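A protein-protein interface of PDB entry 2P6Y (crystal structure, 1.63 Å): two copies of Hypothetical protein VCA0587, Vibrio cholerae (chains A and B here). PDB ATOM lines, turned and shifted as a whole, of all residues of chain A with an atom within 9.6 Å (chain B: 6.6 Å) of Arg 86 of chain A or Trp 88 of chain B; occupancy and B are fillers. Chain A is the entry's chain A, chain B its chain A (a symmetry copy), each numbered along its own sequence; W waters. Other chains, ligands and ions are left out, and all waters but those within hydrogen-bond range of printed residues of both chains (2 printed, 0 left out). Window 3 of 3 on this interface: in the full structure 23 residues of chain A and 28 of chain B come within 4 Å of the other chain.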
ATOM      1  N   LEU A  43      -7.139 -10.369 -20.847  1.00  0.00           N
ATOM      2  CA  LEU A  43      -6.101  -9.348 -20.812  1.00  0.00           C
ATOM      3  C   LEU A  43      -6.756  -7.993 -21.058  1.00  0.00           C
ATOM      4  O   LEU A  43      -7.647  -7.883 -21.900  1.00  0.00           O
ATOM      5  CB  LEU A  43      -5.071  -9.602 -21.919  1.00  0.00           C
ATOM      6  CG  LEU A  43      -4.005  -8.528 -22.183  1.00  0.00           C
ATOM      7  CD1 LEU A  43      -2.977  -8.517 -21.057  1.00  0.00           C
ATOM      8  CD2 LEU A  43      -3.324  -8.814 -23.517  1.00  0.00           C
ATOM      9  N   PRO A  59      -6.292 -17.320 -23.717  1.00  0.00           N
ATOM     10  CA  PRO A  59      -5.247 -17.638 -22.745  1.00  0.00           C
ATOM     11  C   PRO A  59      -3.950 -16.875 -22.981  1.00  0.00           C
ATOM     12  O   PRO A  59      -3.470 -16.758 -24.109  1.00  0.00           O
ATOM     13  CB  PRO A  59      -5.075 -19.147 -22.902  1.00  0.00           C
ATOM     14  CG  PRO A  59      -5.377 -19.365 -24.348  1.00  0.00           C
ATOM     15  CD  PRO A  59      -6.573 -18.470 -24.594  1.00  0.00           C
ATOM     16  N   PHE A  60      -3.392 -16.353 -21.896  1.00  0.00           N
ATOM     17  CA  PHE A  60      -2.138 -15.612 -21.945  1.00  0.00           C
ATOM     18  C   PHE A  60      -1.267 -16.028 -20.776  1.00  0.00           C
ATOM     19  O   PHE A  60      -1.756 -16.179 -19.656  1.00  0.00           O
ATOM     20  CB  PHE A  60      -2.383 -14.110 -21.820  1.00  0.00           C
ATOM     21  CG  PHE A  60      -3.040 -13.491 -23.017  1.00  0.00           C
ATOM     22  CD1 PHE A  60      -2.290 -13.131 -24.133  1.00  0.00           C
ATOM     23  CD2 PHE A  60      -4.408 -13.240 -23.018  1.00  0.00           C
ATOM     24  CE1 PHE A  60      -2.897 -12.521 -25.235  1.00  0.00           C
ATOM     25  CE2 PHE A  60      -5.022 -12.633 -24.113  1.00  0.00           C
ATOM     26  CZ  PHE A  60      -4.264 -12.274 -25.220  1.00  0.00           C
ATOM     27  N   GLU A  61       0.020 -16.212 -21.035  1.00  0.00           N
ATOM     28  CA  GLU A  61       0.958 -16.556 -19.974  1.00  0.00           C
ATOM     29  C   GLU A  61       1.553 -15.231 -19.506  1.00  0.00           C
ATOM     30  O   GLU A  61       1.944 -14.399 -20.330  1.00  0.00           O
ATOM     31  CB  GLU A  61       2.085 -17.443 -20.511  1.00  0.00           C
ATOM     32  CG  GLU A  61       1.644 -18.822 -20.970  1.00  0.00           C
ATOM     33  CD  GLU A  61       1.393 -19.763 -19.812  1.00  0.00           C
ATOM     34  OE1 GLU A  61       2.309 -20.538 -19.459  1.00  0.00           O
ATOM     35  OE2 GLU A  61       0.282 -19.720 -19.246  1.00  0.00           O
ATOM     36  N   ILE A  62       1.595 -15.009 -18.196  1.00  0.00           N
ATOM     37  CA  ILE A  62       2.187 -13.778 -17.684  1.00  0.00           C
ATOM     38  C   ILE A  62       3.700 -13.997 -17.675  1.00  0.00           C
ATOM     39  O   ILE A  62       4.196 -14.889 -16.990  1.00  0.00           O
ATOM     40  CB  ILE A  62       1.718 -13.471 -16.242  1.00  0.00           C
ATOM     41  CG1 ILE A  62       0.195 -13.336 -16.210  1.00  0.00           C
ATOM     42  CG2 ILE A  62       2.388 -12.193 -15.743  1.00  0.00           C
ATOM     43  CD1 ILE A  62      -0.387 -13.136 -14.812  1.00  0.00           C
ATOM     44  N   LEU A  63       4.437 -13.196 -18.440  1.00  0.00           N
ATOM     45  CA  LEU A  63       5.888 -13.351 -18.498  1.00  0.00           C
ATOM     46  C   LEU A  63       6.587 -12.454 -17.496  1.00  0.00           C
ATOM     47  O   LEU A  63       7.568 -12.848 -16.861  1.00  0.00           O
ATOM     48  CB  LEU A  63       6.404 -13.039 -19.905  1.00  0.00           C
ATOM     49  CG  LEU A  63       5.770 -13.840 -21.046  1.00  0.00           C
ATOM     50  CD1 LEU A  63       6.466 -13.468 -22.347  1.00  0.00           C
ATOM     51  CD2 LEU A  63       5.897 -15.331 -20.782  1.00  0.00           C
ATOM     52  N   ALA A  79       3.766  -7.901 -19.438  1.00  0.00           N
ATOM     53  CA  ALA A  79       4.160  -8.522 -20.703  1.00  0.00           C
ATOM     54  C   ALA A  79       3.559  -9.927 -20.644  1.00  0.00           C
ATOM     55  O   ALA A  79       3.784 -10.664 -19.684  1.00  0.00           O
ATOM     56  CB  ALA A  79       5.673  -8.603 -20.828  1.00  0.00           C
ATOM     57  N   VAL A  80       2.782 -10.291 -21.657  1.00  0.00           N
ATOM     58  CA  VAL A  80       2.149 -11.605 -21.694  1.00  0.00           C
ATOM     59  C   VAL A  80       2.382 -12.264 -23.043  1.00  0.00           C
ATOM     60  O   VAL A  80       2.659 -11.585 -24.028  1.00  0.00           O
ATOM     61  CB  VAL A  80       0.620 -11.516 -21.463  1.00  0.00           C
ATOM     62  CG1 VAL A  80       0.330 -10.914 -20.097  1.00  0.00           C
ATOM     63  CG2 VAL A  80      -0.032 -10.683 -22.556  1.00  0.00           C
ATOM     64  N   ALA A  81       2.264 -13.586 -23.084  1.00  0.00           N
ATOM     65  CA  ALA A  81       2.453 -14.316 -24.338  1.00  0.00           C
ATOM     66  C   ALA A  81       1.160 -15.031 -24.707  1.00  0.00           C
ATOM     67  O   ALA A  81       0.492 -15.593 -23.839  1.00  0.00           O
ATOM     68  CB  ALA A  81       3.583 -15.327 -24.196  1.00  0.00           C
ATOM     69  N   ASP A  82       0.803 -15.003 -25.992  1.00  0.00           N
ATOM     70  CA  ASP A  82      -0.412 -15.676 -26.430  1.00  0.00           C
ATOM     71  C   ASP A  82      -0.144 -17.135 -26.791  1.00  0.00           C
ATOM     72  O   ASP A  82       0.967 -17.633 -26.610  1.00  0.00           O
ATOM     73  CB  ASP A  82      -1.064 -14.932 -27.609  1.00  0.00           C
ATOM     74  CG  ASP A  82      -0.174 -14.853 -28.838  1.00  0.00           C
ATOM     75  OD1 ASP A  82       0.667 -15.749 -29.034  1.00  0.00           O
ATOM     76  OD2 ASP A  82      -0.335 -13.897 -29.635  1.00  0.00           O
ATOM     77  N   ALA A  83      -1.170 -17.816 -27.300  1.00  0.00           N
ATOM     78  CA  ALA A  83      -1.064 -19.230 -27.658  1.00  0.00           C
ATOM     79  C   ALA A  83      -0.044 -19.557 -28.746  1.00  0.00           C
ATOM     80  O   ALA A  83       0.319 -20.725 -28.928  1.00  0.00           O
ATOM     81  CB  ALA A  83      -2.438 -19.761 -28.062  1.00  0.00           C
ATOM     82  N   GLN A  84       0.414 -18.540 -29.469  1.00  0.00           N
ATOM     83  CA  GLN A  84       1.401 -18.752 -30.520  1.00  0.00           C
ATOM     84  C   GLN A  84       2.796 -18.341 -30.061  1.00  0.00           C
ATOM     85  O   GLN A  84       3.765 -18.442 -30.819  1.00  0.00           O
ATOM     86  CB  GLN A  84       1.021 -17.970 -31.783  1.00  0.00           C
ATOM     87  CG  GLN A  84      -0.236 -18.482 -32.486  1.00  0.00           C
ATOM     88  CD  GLN A  84      -1.511 -18.147 -31.736  1.00  0.00           C
ATOM     89  OE1 GLN A  84      -1.790 -16.980 -31.457  1.00  0.00           O
ATOM     90  NE2 GLN A  84      -2.296 -19.170 -31.410  1.00  0.00           N
ATOM     91  N   GLY A  85       2.894 -17.882 -28.818  1.00  0.00           N
ATOM     92  CA  GLY A  85       4.179 -17.471 -28.283  1.00  0.00           C
ATOM     93  C   GLY A  85       4.507 -16.003 -28.494  1.00  0.00           C
ATOM     94  O   GLY A  85       5.555 -15.535 -28.041  1.00  0.00           O
ATOM     95  N   ARG A  86       3.633 -15.276 -29.188  1.00  0.00           N
ATOM     96  CA  ARG A  86       3.861 -13.853 -29.438  1.00  0.00           C
ATOM     97  C   ARG A  86       3.605 -13.045 -28.172  1.00  0.00           C
ATOM     98  O   ARG A  86       2.633 -13.285 -27.463  1.00  0.00           O
ATOM     99  CB  ARG A  86       2.944 -13.347 -30.554  1.00  0.00           C
ATOM    100  CG  ARG A  86       3.268 -13.902 -31.929  1.00  0.00           C
ATOM    101  CD  ARG A  86       2.537 -13.120 -33.010  1.00  0.00           C
ATOM    102  NE  ARG A  86       2.973 -13.502 -34.352  1.00  0.00           N
ATOM    103  CZ  ARG A  86       2.792 -14.707 -34.884  1.00  0.00           C
ATOM    104  NH1 ARG A  86       2.179 -15.657 -34.191  1.00  0.00           N
ATOM    105  NH2 ARG A  86       3.228 -14.962 -36.109  1.00  0.00           N
ATOM    106  N   VAL A  87       4.467 -12.070 -27.910  1.00  0.00           N
ATOM    107  CA  VAL A  87       4.336 -11.261 -26.707  1.00  0.00           C
ATOM    108  C   VAL A  87       3.677  -9.904 -26.930  1.00  0.00           C
ATOM    109  O   VAL A  87       3.979  -9.187 -27.893  1.00  0.00           O
ATOM    110  CB  VAL A  87       5.714 -11.080 -26.044  1.00  0.00           C
ATOM    111  CG1 VAL A  87       5.594 -10.246 -24.773  1.00  0.00           C
ATOM    112  CG2 VAL A  87       6.300 -12.454 -25.733  1.00  0.00           C
ATOM    113  N   TRP A  88       2.762  -9.577 -26.023  1.00  0.00           N
ATOM    114  CA  TRP A  88       2.001  -8.333 -26.048  1.00  0.00           C
ATOM    115  C   TRP A  88       2.127  -7.680 -24.683  1.00  0.00           C
ATOM    116  O   TRP A  88       2.429  -8.346 -23.703  1.00  0.00           O
ATOM    117  CB  TRP A  88       0.525  -8.628 -26.318  1.00  0.00           C
ATOM    118  CG  TRP A  88       0.302  -9.423 -27.565  1.00  0.00           C
ATOM    119  CD1 TRP A  88       0.373 -10.777 -27.702  1.00  0.00           C
ATOM    120  CD2 TRP A  88       0.034  -8.897 -28.870  1.00  0.00           C
ATOM    121  NE1 TRP A  88       0.170 -11.132 -29.018  1.00  0.00           N
ATOM    122  CE2 TRP A  88      -0.039  -9.994 -29.756  1.00  0.00           C
ATOM    123  CE3 TRP A  88      -0.148  -7.604 -29.378  1.00  0.00           C
ATOM    124  CZ2 TRP A  88      -0.287  -9.839 -31.125  1.00  0.00           C
ATOM    125  CZ3 TRP A  88      -0.396  -7.449 -30.743  1.00  0.00           C
ATOM    126  CH2 TRP A  88      -0.462  -8.562 -31.596  1.00  0.00           C
ATOM    127  N   GLY A  89       1.880  -6.381 -24.605  1.00  0.00           N
ATOM    128  CA  GLY A  89       1.993  -5.751 -23.307  1.00  0.00           C
ATOM    129  C   GLY A  89       1.656  -4.283 -23.272  1.00  0.00           C
ATOM    130  O   GLY A  89       1.465  -3.649 -24.308  1.00  0.00           O
ATOM    131  N   LEU B  43      15.848 -22.110 -28.101  1.00  0.00           N
ATOM    132  CA  LEU B  43      14.714 -21.742 -27.265  1.00  0.00           C
ATOM    133  C   LEU B  43      13.743 -22.918 -27.235  1.00  0.00           C
ATOM    134  O   LEU B  43      13.521 -23.561 -28.260  1.00  0.00           O
ATOM    135  CB  LEU B  43      13.992 -20.527 -27.857  1.00  0.00           C
ATOM    136  CG  LEU B  43      12.651 -20.103 -27.238  1.00  0.00           C
ATOM    137  CD1 LEU B  43      12.879 -19.460 -25.874  1.00  0.00           C
ATOM    138  CD2 LEU B  43      11.954 -19.121 -28.175  1.00  0.00           C
ATOM    139  N   ILE B  45       9.982 -23.551 -25.350  1.00  0.00           N
ATOM    140  CA  ILE B  45       8.941 -23.110 -24.439  1.00  0.00           C
ATOM    141  C   ILE B  45       7.583 -23.745 -24.692  1.00  0.00           C
ATOM    142  O   ILE B  45       7.270 -24.143 -25.818  1.00  0.00           O
ATOM    143  CB  ILE B  45       8.755 -21.571 -24.524  1.00  0.00           C
ATOM    144  CG1 ILE B  45       8.611 -21.142 -25.990  1.00  0.00           C
ATOM    145  CG2 ILE B  45       9.923 -20.868 -23.852  1.00  0.00           C
ATOM    146  CD1 ILE B  45       8.209 -19.684 -26.177  1.00  0.00           C
ATOM    147  N   LEU B  47       3.637 -23.111 -24.813  1.00  0.00           N
ATOM    148  CA  LEU B  47       2.840 -21.922 -25.078  1.00  0.00           C
ATOM    149  C   LEU B  47       1.581 -21.754 -24.227  1.00  0.00           C
ATOM    150  O   LEU B  47       1.230 -22.632 -23.442  1.00  0.00           O
ATOM    151  CB  LEU B  47       2.526 -21.862 -26.580  1.00  0.00           C
ATOM    152  CG  LEU B  47       3.785 -22.076 -27.442  1.00  0.00           C
ATOM    153  CD1 LEU B  47       3.434 -21.974 -28.919  1.00  0.00           C
ATOM    154  CD2 LEU B  47       4.856 -21.036 -27.082  1.00  0.00           C
ATOM    155  N   LEU B  54       7.194 -24.684 -28.629  1.00  0.00           N
ATOM    156  CA  LEU B  54       8.012 -24.082 -29.664  1.00  0.00           C
ATOM    157  C   LEU B  54       9.479 -24.275 -29.351  1.00  0.00           C
ATOM    158  O   LEU B  54       9.944 -23.914 -28.268  1.00  0.00           O
ATOM    159  CB  LEU B  54       7.719 -22.580 -29.768  1.00  0.00           C
ATOM    160  CG  LEU B  54       8.558 -21.743 -30.739  1.00  0.00           C
ATOM    161  CD1 LEU B  54       8.319 -22.195 -32.172  1.00  0.00           C
ATOM    162  CD2 LEU B  54       8.191 -20.271 -30.586  1.00  0.00           C
ATOM    163  N   PHE B  60      18.740 -15.772 -29.660  1.00  0.00           N
ATOM    164  CA  PHE B  60      17.709 -15.067 -28.909  1.00  0.00           C
ATOM    165  C   PHE B  60      18.348 -14.356 -27.733  1.00  0.00           C
ATOM    166  O   PHE B  60      19.212 -14.916 -27.058  1.00  0.00           O
ATOM    167  CB  PHE B  60      16.676 -16.042 -28.347  1.00  0.00           C
ATOM    168  CG  PHE B  60      15.790 -16.668 -29.383  1.00  0.00           C
ATOM    169  CD1 PHE B  60      14.677 -15.991 -29.869  1.00  0.00           C
ATOM    170  CD2 PHE B  60      16.055 -17.950 -29.852  1.00  0.00           C
ATOM    171  CE1 PHE B  60      13.831 -16.588 -30.808  1.00  0.00           C
ATOM    172  CE2 PHE B  60      15.218 -18.554 -30.790  1.00  0.00           C
ATOM    173  CZ  PHE B  60      14.106 -17.870 -31.265  1.00  0.00           C
ATOM    174  N   LEU B  63      15.408 -11.388 -22.389  1.00  0.00           N
ATOM    175  CA  LEU B  63      15.010 -10.071 -21.898  1.00  0.00           C
ATOM    176  C   LEU B  63      14.589 -10.120 -20.442  1.00  0.00           C
ATOM    177  O   LEU B  63      14.896  -9.221 -19.658  1.00  0.00           O
ATOM    178  CB  LEU B  63      13.861  -9.510 -22.740  1.00  0.00           C
ATOM    179  CG  LEU B  63      14.112  -9.426 -24.248  1.00  0.00           C
ATOM    180  CD1 LEU B  63      12.910  -8.765 -24.906  1.00  0.00           C
ATOM    181  CD2 LEU B  63      15.378  -8.633 -24.532  1.00  0.00           C
ATOM    182  N   ILE B  78       9.733 -17.151 -19.513  1.00  0.00           N
ATOM    183  CA  ILE B  78      10.778 -16.363 -20.146  1.00  0.00           C
ATOM    184  C   ILE B  78      10.278 -15.498 -21.302  1.00  0.00           C
ATOM    185  O   ILE B  78       9.282 -15.826 -21.947  1.00  0.00           O
ATOM    186  CB  ILE B  78      11.891 -17.320 -20.667  1.00  0.00           C
ATOM    187  CG1 ILE B  78      13.170 -16.550 -20.995  1.00  0.00           C
ATOM    188  CG2 ILE B  78      11.394 -18.086 -21.899  1.00  0.00           C
ATOM    189  CD1 ILE B  78      14.343 -17.455 -21.372  1.00  0.00           C
ATOM    190  N   ALA B  79      10.958 -14.376 -21.524  1.00  0.00           N
ATOM    191  CA  ALA B  79      10.657 -13.486 -22.645  1.00  0.00           C
ATOM    192  C   ALA B  79      11.994 -13.311 -23.366  1.00  0.00           C
ATOM    193  O   ALA B  79      12.994 -12.946 -22.749  1.00  0.00           O
ATOM    194  CB  ALA B  79      10.145 -12.140 -22.157  1.00  0.00           C
ATOM    195  N   VAL B  80      12.017 -13.589 -24.664  1.00  0.00           N
ATOM    196  CA  VAL B  80      13.244 -13.469 -25.445  1.00  0.00           C
ATOM    197  C   VAL B  80      12.983 -12.679 -26.716  1.00  0.00           C
ATOM    198  O   VAL B  80      11.845 -12.585 -27.169  1.00  0.00           O
ATOM    199  CB  VAL B  80      13.810 -14.852 -25.848  1.00  0.00           C
ATOM    200  CG1 VAL B  80      14.143 -15.665 -24.608  1.00  0.00           C
ATOM    201  CG2 VAL B  80      12.809 -15.601 -26.716  1.00  0.00           C
ATOM    202  N   ALA B  81      14.040 -12.117 -27.292  1.00  0.00           N
ATOM    203  CA  ALA B  81      13.899 -11.349 -28.529  1.00  0.00           C
ATOM    204  C   ALA B  81      14.707 -12.017 -29.634  1.00  0.00           C
ATOM    205  O   ALA B  81      15.824 -12.477 -29.396  1.00  0.00           O
ATOM    206  CB  ALA B  81      14.386  -9.921 -28.322  1.00  0.00           C
ATOM    207  N   ASP B  82      14.139 -12.080 -30.839  1.00  0.00           N
ATOM    208  CA  ASP B  82      14.850 -12.690 -31.954  1.00  0.00           C
ATOM    209  C   ASP B  82      15.719 -11.670 -32.687  1.00  0.00           C
ATOM    210  O   ASP B  82      15.829 -10.519 -32.265  1.00  0.00           O
ATOM    211  CB  ASP B  82      13.874 -13.377 -32.926  1.00  0.00           C
ATOM    212  CG  ASP B  82      12.875 -12.419 -33.553  1.00  0.00           C
ATOM    213  OD1 ASP B  82      13.193 -11.226 -33.703  1.00  0.00           O
ATOM    214  OD2 ASP B  82      11.765 -12.871 -33.927  1.00  0.00           O
ATOM    215  N   GLY B  85      14.228  -8.328 -33.402  1.00  0.00           N
ATOM    216  CA  GLY B  85      13.749  -7.549 -32.275  1.00  0.00           C
ATOM    217  C   GLY B  85      12.376  -7.955 -31.769  1.00  0.00           C
ATOM    218  O   GLY B  85      11.889  -7.389 -30.787  1.00  0.00           O
ATOM    219  N   ARG B  86      11.740  -8.918 -32.435  1.00  0.00           N
ATOM    220  CA  ARG B  86      10.416  -9.379 -32.019  1.00  0.00           C
ATOM    221  C   ARG B  86      10.524 -10.245 -30.771  1.00  0.00           C
ATOM    222  O   ARG B  86      11.408 -11.090 -30.671  1.00  0.00           O
ATOM    223  CB  ARG B  86       9.749 -10.185 -33.137  1.00  0.00           C
ATOM    224  CG  ARG B  86       9.362  -9.365 -34.354  1.00  0.00           C
ATOM    225  CD  ARG B  86       8.435 -10.157 -35.263  1.00  0.00           C
ATOM    226  NE  ARG B  86       7.892  -9.334 -36.343  1.00  0.00           N
ATOM    227  CZ  ARG B  86       8.623  -8.787 -37.308  1.00  0.00           C
ATOM    228  NH1 ARG B  86       9.936  -8.973 -37.338  1.00  0.00           N
ATOM    229  NH2 ARG B  86       8.041  -8.049 -38.243  1.00  0.00           N
ATOM    230  N   VAL B  87       9.602 -10.049 -29.836  1.00  0.00           N
ATOM    231  CA  VAL B  87       9.635 -10.797 -28.587  1.00  0.00           C
ATOM    232  C   VAL B  87       8.676 -11.982 -28.539  1.00  0.00           C
ATOM    233  O   VAL B  87       7.512 -11.890 -28.949  1.00  0.00           O
ATOM    234  CB  VAL B  87       9.371  -9.851 -27.401  1.00  0.00           C
ATOM    235  CG1 VAL B  87       9.416 -10.616 -26.083  1.00  0.00           C
ATOM    236  CG2 VAL B  87      10.414  -8.737 -27.414  1.00  0.00           C
ATOM    237  N   TRP B  88       9.199 -13.097 -28.039  1.00  0.00           N
ATOM    238  CA  TRP B  88       8.465 -14.351 -27.909  1.00  0.00           C
ATOM    239  C   TRP B  88       8.618 -14.836 -26.479  1.00  0.00           C
ATOM    240  O   TRP B  88       9.547 -14.445 -25.787  1.00  0.00           O
ATOM    241  CB  TRP B  88       9.055 -15.402 -28.851  1.00  0.00           C
ATOM    242  CG  TRP B  88       9.108 -14.952 -30.276  1.00  0.00           C
ATOM    243  CD1 TRP B  88      10.077 -14.195 -30.865  1.00  0.00           C
ATOM    244  CD2 TRP B  88       8.110 -15.180 -31.276  1.00  0.00           C
ATOM    245  NE1 TRP B  88       9.742 -13.932 -32.176  1.00  0.00           N
ATOM    246  CE2 TRP B  88       8.537 -14.525 -32.452  1.00  0.00           C
ATOM    247  CE3 TRP B  88       6.892 -15.873 -31.293  1.00  0.00           C
ATOM    248  CZ2 TRP B  88       7.788 -14.542 -33.635  1.00  0.00           C
ATOM    249  CZ3 TRP B  88       6.145 -15.890 -32.472  1.00  0.00           C
ATOM    250  CH2 TRP B  88       6.599 -15.228 -33.624  1.00  0.00           C
ATOM    251  N   GLY B  89       7.721 -15.703 -26.032  1.00  0.00           N
ATOM    252  CA  GLY B  89       7.861 -16.175 -24.671  1.00  0.00           C
ATOM    253  C   GLY B  89       6.840 -17.193 -24.234  1.00  0.00           C
ATOM    254  O   GLY B  89       5.869 -17.464 -24.938  1.00  0.00           O
ATOM    255  N   GLY B  90       7.075 -17.756 -23.054  1.00  0.00           N
ATOM    256  CA  GLY B  90       6.174 -18.749 -22.510  1.00  0.00           C
ATOM    257  C   GLY B  90       6.797 -19.459 -21.326  1.00  0.00           C
ATOM    258  O   GLY B  90       7.719 -18.943 -20.688  1.00  0.00           O
HETATM  259  O   HOH W   1       3.111 -18.584 -24.826  1.00  0.00           O
HETATM  260  O   HOH W   2       2.284 -23.085 -20.926  1.00  0.00           O
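The backbone NH (N) of Gly 89 of chain B sits at hydrogen-bond distance from the backbone carbonyl oxygen (O) of Gly 85 of chain A, at 3.0 Å. O of Val 87 of chain B sits at hydrogen-bond distance from N of Val 87 of chain A (3.2 Å).
N of Gln 84 of chain A sits at hydrogen-bond distance from OD1 of Asp 82 of chain A. The backbone NH (N) of Gly 85 of chain A lies within hydrogen-bond range of the side-chain carboxylate (OD1) of Asp 82 of chain A (3.1 Å). The backbone NH (N) of Arg 86 of chain A lies within hydrogen-bond range of the side-chain carboxylate (OD1) of Asp 82 of chain A, 3.0 Å away. The backbone carbonyl oxygen (O) of Ala 79 of chain B is in hydrogen-bond range of the backbone NH (N) of Leu 63 of chain B. The backbone NH (N) of Ile 78 of chain B sits at hydrogen-bond distance from the backbone carbonyl oxygen (O) of Gly 90 of chain B, 2.9 Å away. The backbone NH of Trp 88 of chain B sits at hydrogen-bond distance from the backbone carbonyl oxygen of Val 80 of chain B (2.8 Å).
Among the printed residues, pairs that only touch across the chains: Leu 63 of chain A with Ile 78 of chain B (3.6 Å), Leu 63 of chain A with Ala 79 of chain B (3.9 Å), Leu 63 of chain A with Gly 89 of chain B (3.8 Å), Leu 63 of chain A with Gly 90 of chain B (3.5 Å), Ala 81 of chain A with Gly 89 of chain B (3.2 Å), Ala 83 of chain A with Leu 47 of chain B (3.4 Å), Gln 84 of chain A with Leu 47 of chain B (3.9 Å), Gln 84 of chain A with Trp 88 of chain B (3.9 Å), Gly 85 of chain A with Leu 47 of chain B (3.8 Å), Gly 85 of chain A with Trp 88 of chain B (3.1 Å), Arg 86 of chain A with Trp 88 of chain B (3.5 Å), Val 87 of chain A with Trp 88 of chain B (3.4 Å) and Val 87 of chain A with Gly 89 of chain B (3.6 Å).
Of the printed residues of chain B, Ala 81 of chain A touches Gly 89. Of the printed residues of chain B, Val 87 of chain A touches Val 87 (3.2 Å), Trp 88 (3.4 Å) and Gly 89 (3.6 Å). Of chain A, only Leu 63 (3.9 Å) comes within 4 Å of Ala 79 of chain B. Val 80 of chain B touches none of the printed residues of chain A. Printed residues of chain A within 4 Å of Val 87 of chain B: Val 87. Trp 88 of chain B touches just these residues of chain A: Gln 84, Gly 85, Arg 86 and Val 87. Of the printed residues of chain A, Gly 90 of chain B touches Leu 63 (3.5 Å). The nearest residue of chain B that does not touch Arg 86 of chain A is Val 87 of chain B (4.1 Å). The nearest residue of chain A that does not touch Trp 88 of chain B is Leu 63 of chain A (4.7 Å). The nearest printed residue of chain B that does not touch Val 87 of chain A is Ala 79 of chain B (5.3 Å).
Of the 17 printed residues of chain A, 7 touch a printed residue of chain B. Hydrophobic or aromatic side chains of chain A that line the printed part of chain B: Leu 63, Ala 81 and Val 87. Among the printed residues, 15 pairs touch across the chains.
Leu 63 of chain A touches Ala 79 of chain B, but with the chains exchanged Ala 79 of chain A does not touch Leu 63 of chain B (8.3 Å). Ala 81 of chain A touches Gly 89 of chain B, but with the chains exchanged Gly 89 of chain A does not touch Ala 81 of chain B (13.5 Å). Gly 85 of chain A touches Trp 88 of chain B, but with the chains exchanged Trp 88 of chain A does not touch Gly 85 of chain B (10.5 Å). Val 87 of chain A touches Trp 88 of chain B, but with the chains exchanged Trp 88 of chain A does not touch Val 87 of chain B (6.0 Å). Positions printed for both chains: 43, 60, 63, 79, 80, 81, 82, 85, 86, 87, 88 and 89. Of the 15 pairs that touch across the chains among the printed residues, 1 has its exchanged pair printed and touching as well.
Water W2 bridges O of Leu 47 of chain B (2.8 Å) and OE1 of Glu 61 of chain A (2.9 Å). Water W1 bridges the backbone carbonyl oxygen (O) of Asp 82 of chain A and the backbone carbonyl oxygen (O) of Gly 89 of chain B.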
